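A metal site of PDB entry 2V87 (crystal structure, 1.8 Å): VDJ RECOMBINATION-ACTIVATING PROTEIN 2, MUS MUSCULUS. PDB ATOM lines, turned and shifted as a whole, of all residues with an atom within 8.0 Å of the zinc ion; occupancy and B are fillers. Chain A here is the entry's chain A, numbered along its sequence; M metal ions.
The zinc ion is bound by ND1 of His 50, SG of Cys 18, SG of Cys 14 and SG of Cys 53.
The zinc ion has four donor atoms within binding distance.
NE2 of His 50 lies within hydrogen-bond range of O of Tyr 10, 2.7 Å away.
The side-chain sulfur of Cys 53 sits close to the backbone NH of Asp 19 (3.5 Å).
The side-chain sulfur (SG) of Cys 15 sits at hydrogen-bond distance from the backbone NH (N) of Cys 18 (3.5 Å).
SG of Cys 18 lies close to N of Val 20.
Four residues have an atom within 4 Å of the zinc ion: Cys 14, Cys 18, His 50 and Cys 53.
Along chain A the residues within 4 Å of the zinc ion span positions 14 to 53.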
ATOM      1  N   TYR A  10      -5.534 -14.112  -8.436  1.00  0.00           N
ATOM      2  CA  TYR A  10      -4.739 -13.468  -7.391  1.00  0.00           C
ATOM      3  C   TYR A  10      -5.151 -13.855  -5.974  1.00  0.00           C
ATOM      4  O   TYR A  10      -4.311 -13.883  -5.071  1.00  0.00           O
ATOM      5  CB  TYR A  10      -4.817 -11.943  -7.505  1.00  0.00           C
ATOM      6  CG  TYR A  10      -3.984 -11.355  -8.617  1.00  0.00           C
ATOM      7  CD1 TYR A  10      -4.526 -11.118  -9.872  1.00  0.00           C
ATOM      8  CD2 TYR A  10      -2.651 -11.017  -8.391  1.00  0.00           C
ATOM      9  CE1 TYR A  10      -3.761 -10.558 -10.893  1.00  0.00           C
ATOM     10  CE2 TYR A  10      -1.882 -10.456  -9.398  1.00  0.00           C
ATOM     11  CZ  TYR A  10      -2.434 -10.229 -10.650  1.00  0.00           C
ATOM     12  OH  TYR A  10      -1.671  -9.677 -11.640  1.00  0.00           O
ATOM     13  N   TRP A  11      -6.429 -14.145  -5.787  1.00  0.00           N
ATOM     14  CA  TRP A  11      -6.934 -14.456  -4.456  1.00  0.00           C
ATOM     15  C   TRP A  11      -7.134 -15.927  -4.128  1.00  0.00           C
ATOM     16  O   TRP A  11      -8.077 -16.299  -3.438  1.00  0.00           O
ATOM     17  CB  TRP A  11      -8.211 -13.662  -4.211  1.00  0.00           C
ATOM     18  CG  TRP A  11      -7.997 -12.214  -4.476  1.00  0.00           C
ATOM     19  CD1 TRP A  11      -8.552 -11.465  -5.473  1.00  0.00           C
ATOM     20  CD2 TRP A  11      -7.103 -11.338  -3.760  1.00  0.00           C
ATOM     21  NE1 TRP A  11      -8.064 -10.178  -5.418  1.00  0.00           N
ATOM     22  CE2 TRP A  11      -7.179 -10.078  -4.384  1.00  0.00           C
ATOM     23  CE3 TRP A  11      -6.255 -11.507  -2.657  1.00  0.00           C
ATOM     24  CZ2 TRP A  11      -6.426  -8.984  -3.945  1.00  0.00           C
ATOM     25  CZ3 TRP A  11      -5.510 -10.423  -2.215  1.00  0.00           C
ATOM     26  CH2 TRP A  11      -5.603  -9.175  -2.863  1.00  0.00           C
ATOM     27  N   ILE A  12      -6.219 -16.756  -4.604  1.00  0.00           N
ATOM     28  CA  ILE A  12      -6.256 -18.175  -4.355  1.00  0.00           C
ATOM     29  C   ILE A  12      -5.491 -18.434  -3.057  1.00  0.00           C
ATOM     30  O   ILE A  12      -4.833 -17.540  -2.534  1.00  0.00           O
ATOM     31  CB  ILE A  12      -5.510 -18.962  -5.451  1.00  0.00           C
ATOM     32  CG1 ILE A  12      -4.046 -18.502  -5.493  1.00  0.00           C
ATOM     33  CG2 ILE A  12      -6.178 -18.739  -6.806  1.00  0.00           C
ATOM     34  CD1 ILE A  12      -3.129 -19.373  -6.324  1.00  0.00           C
ATOM     35  N   THR A  13      -5.594 -19.657  -2.561  1.00  0.00           N
ATOM     36  CA  THR A  13      -4.836 -20.064  -1.379  1.00  0.00           C
ATOM     37  C   THR A  13      -3.711 -20.810  -2.081  1.00  0.00           C
ATOM     38  O   THR A  13      -3.877 -21.950  -2.490  1.00  0.00           O
ATOM     39  CB  THR A  13      -5.663 -21.018  -0.485  1.00  0.00           C
ATOM     40  OG1 THR A  13      -6.780 -20.296   0.064  1.00  0.00           O
ATOM     41  CG2 THR A  13      -4.811 -21.565   0.643  1.00  0.00           C
ATOM     42  N   CYS A  14      -2.570 -20.144  -2.246  1.00  0.00           N
ATOM     43  CA  CYS A  14      -1.445 -20.711  -2.971  1.00  0.00           C
ATOM     44  C   CYS A  14      -0.692 -21.887  -2.371  1.00  0.00           C
ATOM     45  O   CYS A  14      -0.022 -22.627  -3.088  1.00  0.00           O
ATOM     46  CB  CYS A  14      -0.433 -19.608  -3.339  1.00  0.00           C
ATOM     47  SG  CYS A  14       0.678 -19.115  -2.014  1.00  0.00           S
ATOM     48  N   CYS A  15      -0.777 -22.046  -1.059  1.00  0.00           N
ATOM     49  CA  CYS A  15      -0.091 -23.142  -0.392  1.00  0.00           C
ATOM     50  C   CYS A  15      -0.694 -23.346   0.997  1.00  0.00           C
ATOM     51  O   CYS A  15      -1.470 -22.530   1.456  1.00  0.00           O
ATOM     52  CB  CYS A  15       1.419 -22.847  -0.292  1.00  0.00           C
ATOM     53  SG  CYS A  15       1.858 -21.455   0.766  1.00  0.00           S
ATOM     54  N   PRO A  16      -0.338 -24.440   1.678  1.00  0.00           N
ATOM     55  CA  PRO A  16      -0.868 -24.735   3.020  1.00  0.00           C
ATOM     56  C   PRO A  16      -0.681 -23.634   4.069  1.00  0.00           C
ATOM     57  O   PRO A  16      -1.427 -23.583   5.033  1.00  0.00           O
ATOM     58  CB  PRO A  16      -0.151 -26.026   3.391  1.00  0.00           C
ATOM     59  CG  PRO A  16       0.005 -26.709   2.069  1.00  0.00           C
ATOM     60  CD  PRO A  16       0.491 -25.563   1.204  1.00  0.00           C
ATOM     61  N   THR A  17       0.309 -22.771   3.873  1.00  0.00           N
ATOM     62  CA  THR A  17       0.565 -21.701   4.836  1.00  0.00           C
ATOM     63  C   THR A  17       0.278 -20.308   4.280  1.00  0.00           C
ATOM     64  O   THR A  17       0.655 -19.312   4.876  1.00  0.00           O
ATOM     65  CB  THR A  17       2.020 -21.746   5.329  1.00  0.00           C
ATOM     66  OG1 THR A  17       2.904 -21.640   4.202  1.00  0.00           O
ATOM     67  CG2 THR A  17       2.311 -23.061   6.059  1.00  0.00           C
ATOM     68  N   CYS A  18      -0.405 -20.251   3.140  1.00  0.00           N
ATOM     69  CA  CYS A  18      -0.713 -18.979   2.476  1.00  0.00           C
ATOM     70  C   CYS A  18      -1.317 -17.943   3.400  1.00  0.00           C
ATOM     71  O   CYS A  18      -2.303 -18.198   4.090  1.00  0.00           O
ATOM     72  CB  CYS A  18      -1.647 -19.236   1.292  1.00  0.00           C
ATOM     73  SG  CYS A  18      -2.128 -17.755   0.382  1.00  0.00           S
ATOM     74  N   ASP A  19      -0.719 -16.750   3.408  1.00  0.00           N
ATOM     75  CA  ASP A  19      -1.146 -15.629   4.238  1.00  0.00           C
ATOM     76  C   ASP A  19      -1.901 -14.557   3.451  1.00  0.00           C
ATOM     77  O   ASP A  19      -2.448 -13.637   4.035  1.00  0.00           O
ATOM     78  CB  ASP A  19       0.070 -14.959   4.887  1.00  0.00           C
ATOM     79  CG  ASP A  19       0.582 -15.701   6.098  1.00  0.00           C
ATOM     80  OD1 ASP A  19       1.767 -15.521   6.426  1.00  0.00           O
ATOM     81  OD2 ASP A  19      -0.201 -16.434   6.723  1.00  0.00           O
ATOM     82  N   VAL A  20      -1.920 -14.679   2.130  1.00  0.00           N
ATOM     83  CA  VAL A  20      -2.618 -13.700   1.301  1.00  0.00           C
ATOM     84  C   VAL A  20      -4.112 -13.929   1.337  1.00  0.00           C
ATOM     85  O   VAL A  20      -4.601 -14.990   0.962  1.00  0.00           O
ATOM     86  CB  VAL A  20      -2.098 -13.746  -0.156  1.00  0.00           C
ATOM     87  CG1 VAL A  20      -2.940 -12.821  -1.041  1.00  0.00           C
ATOM     88  CG2 VAL A  20      -0.649 -13.315  -0.206  1.00  0.00           C
ATOM     89  N   ASP A  21      -4.840 -12.914   1.788  1.00  0.00           N
ATOM     90  CA  ASP A  21      -6.295 -12.982   1.889  1.00  0.00           C
ATOM     91  C   ASP A  21      -6.904 -11.717   1.305  1.00  0.00           C
ATOM     92  O   ASP A  21      -6.489 -10.610   1.642  1.00  0.00           O
ATOM     93  CB  ASP A  21      -6.679 -13.161   3.369  1.00  0.00           C
ATOM     94  CG  ASP A  21      -8.164 -13.365   3.576  1.00  0.00           C
ATOM     95  OD1 ASP A  21      -8.523 -13.994   4.585  1.00  0.00           O
ATOM     96  OD2 ASP A  21      -8.960 -12.883   2.755  1.00  0.00           O
ATOM     97  N   PRO A  36      -1.304  -8.678  -4.933  1.00  0.00           N
ATOM     98  CA  PRO A  36      -0.122  -9.422  -4.495  1.00  0.00           C
ATOM     99  C   PRO A  36       0.760  -9.882  -5.653  1.00  0.00           C
ATOM    100  O   PRO A  36       0.274 -10.306  -6.696  1.00  0.00           O
ATOM    101  CB  PRO A  36      -0.720 -10.595  -3.732  1.00  0.00           C
ATOM    102  CG  PRO A  36      -1.990 -10.854  -4.477  1.00  0.00           C
ATOM    103  CD  PRO A  36      -2.540  -9.458  -4.685  1.00  0.00           C
ATOM    104  N   ALA A  37       2.071  -9.784  -5.444  1.00  0.00           N
ATOM    105  CA  ALA A  37       3.015 -10.216  -6.458  1.00  0.00           C
ATOM    106  C   ALA A  37       2.949 -11.739  -6.478  1.00  0.00           C
ATOM    107  O   ALA A  37       2.787 -12.371  -5.435  1.00  0.00           O
ATOM    108  CB  ALA A  37       4.423  -9.750  -6.100  1.00  0.00           C
ATOM    109  N   MET A  38       3.058 -12.318  -7.665  1.00  0.00           N
ATOM    110  CA  MET A  38       2.992 -13.764  -7.787  1.00  0.00           C
ATOM    111  C   MET A  38       4.084 -14.292  -8.704  1.00  0.00           C
ATOM    112  O   MET A  38       4.650 -13.553  -9.510  1.00  0.00           O
ATOM    113  CB  MET A  38       1.613 -14.172  -8.317  1.00  0.00           C
ATOM    114  CG  MET A  38       0.466 -13.761  -7.398  1.00  0.00           C
ATOM    115  SD  MET A  38      -1.136 -14.453  -7.887  1.00  0.00           S
ATOM    116  CE  MET A  38      -1.011 -16.088  -7.162  1.00  0.00           C
ATOM    117  N   TRP A  48       0.417 -21.126  -9.856  1.00  0.00           N
ATOM    118  CA  TRP A  48       0.832 -19.829  -9.346  1.00  0.00           C
ATOM    119  C   TRP A  48       0.844 -19.747  -7.823  1.00  0.00           C
ATOM    120  O   TRP A  48      -0.023 -20.296  -7.166  1.00  0.00           O
ATOM    121  CB  TRP A  48      -0.101 -18.735  -9.888  1.00  0.00           C
ATOM    122  CG  TRP A  48       0.043 -18.474 -11.361  1.00  0.00           C
ATOM    123  CD1 TRP A  48      -0.669 -19.066 -12.372  1.00  0.00           C
ATOM    124  CD2 TRP A  48       0.929 -17.547 -11.976  1.00  0.00           C
ATOM    125  NE1 TRP A  48      -0.286 -18.539 -13.583  1.00  0.00           N
ATOM    126  CE2 TRP A  48       0.702 -17.599 -13.369  1.00  0.00           C
ATOM    127  CE3 TRP A  48       1.902 -16.655 -11.485  1.00  0.00           C
ATOM    128  CZ2 TRP A  48       1.408 -16.814 -14.279  1.00  0.00           C
ATOM    129  CZ3 TRP A  48       2.608 -15.869 -12.394  1.00  0.00           C
ATOM    130  CH2 TRP A  48       2.352 -15.952 -13.778  1.00  0.00           C
ATOM    131  N   VAL A  49       1.831 -19.054  -7.267  1.00  0.00           N
ATOM    132  CA  VAL A  49       1.922 -18.862  -5.824  1.00  0.00           C
ATOM    133  C   VAL A  49       2.254 -17.408  -5.556  1.00  0.00           C
ATOM    134  O   VAL A  49       2.780 -16.717  -6.413  1.00  0.00           O
ATOM    135  CB  VAL A  49       3.024 -19.753  -5.172  1.00  0.00           C
ATOM    136  CG1 VAL A  49       2.690 -21.225  -5.344  1.00  0.00           C
ATOM    137  CG2 VAL A  49       4.392 -19.420  -5.756  1.00  0.00           C
ATOM    138  N   HIS A  50       1.916 -16.940  -4.355  1.00  0.00           N
ATOM    139  CA  HIS A  50       2.218 -15.563  -3.985  1.00  0.00           C
ATOM    140  C   HIS A  50       3.682 -15.543  -3.572  1.00  0.00           C
ATOM    141  O   HIS A  50       4.126 -16.385  -2.796  1.00  0.00           O
ATOM    142  CB  HIS A  50       1.340 -15.119  -2.798  1.00  0.00           C
ATOM    143  CG  HIS A  50      -0.129 -15.198  -3.065  1.00  0.00           C
ATOM    144  ND1 HIS A  50      -0.958 -16.086  -2.409  1.00  0.00           N
ATOM    145  CD2 HIS A  50      -0.920 -14.503  -3.913  1.00  0.00           C
ATOM    146  CE1 HIS A  50      -2.197 -15.926  -2.848  1.00  0.00           C
ATOM    147  NE2 HIS A  50      -2.202 -14.979  -3.768  1.00  0.00           N
ATOM    148  N   ALA A  51       4.433 -14.583  -4.099  1.00  0.00           N
ATOM    149  CA  ALA A  51       5.847 -14.484  -3.769  1.00  0.00           C
ATOM    150  C   ALA A  51       6.086 -14.321  -2.264  1.00  0.00           C
ATOM    151  O   ALA A  51       7.026 -14.899  -1.717  1.00  0.00           O
ATOM    152  CB  ALA A  51       6.478 -13.320  -4.525  1.00  0.00           C
ATOM    153  N   GLN A  52       5.247 -13.548  -1.589  1.00  0.00           N
ATOM    154  CA  GLN A  52       5.415 -13.331  -0.152  1.00  0.00           C
ATOM    155  C   GLN A  52       5.238 -14.623   0.638  1.00  0.00           C
ATOM    156  O   GLN A  52       5.914 -14.836   1.632  1.00  0.00           O
ATOM    157  CB  GLN A  52       4.428 -12.282   0.381  1.00  0.00           C
ATOM    158  CG  GLN A  52       4.823 -11.731   1.756  1.00  0.00           C
ATOM    159  CD  GLN A  52       3.835 -10.715   2.307  1.00  0.00           C
ATOM    160  OE1 GLN A  52       3.048 -10.132   1.555  1.00  0.00           O
ATOM    161  NE2 GLN A  52       3.882 -10.487   3.611  1.00  0.00           N
ATOM    162  N   CYS A  53       4.329 -15.471   0.193  1.00  0.00           N
ATOM    163  CA  CYS A  53       4.068 -16.730   0.876  1.00  0.00           C
ATOM    164  C   CYS A  53       5.257 -17.680   0.753  1.00  0.00           C
ATOM    165  O   CYS A  53       5.359 -18.642   1.498  1.00  0.00           O
ATOM    166  CB  CYS A  53       2.805 -17.390   0.310  1.00  0.00           C
ATOM    167  SG  CYS A  53       1.319 -16.394   0.566  1.00  0.00           S
ATOM    168  N   MET A  54       6.165 -17.379  -0.178  1.00  0.00           N
ATOM    169  CA  MET A  54       7.356 -18.194  -0.394  1.00  0.00           C
ATOM    170  C   MET A  54       8.555 -17.600   0.339  1.00  0.00           C
ATOM    171  O   MET A  54       9.646 -18.122   0.268  1.00  0.00           O
ATOM    172  CB  MET A  54       7.687 -18.256  -1.891  1.00  0.00           C
ATOM    173  CG  MET A  54       6.596 -18.862  -2.758  1.00  0.00           C
ATOM    174  SD  MET A  54       6.291 -20.583  -2.375  1.00  0.00           S
ATOM    175  CE  MET A  54       4.719 -20.486  -1.538  1.00  0.00           C
HETATM  176 ZN    ZN M   1      -0.233 -17.346  -0.854  1.00  0.00          ZN
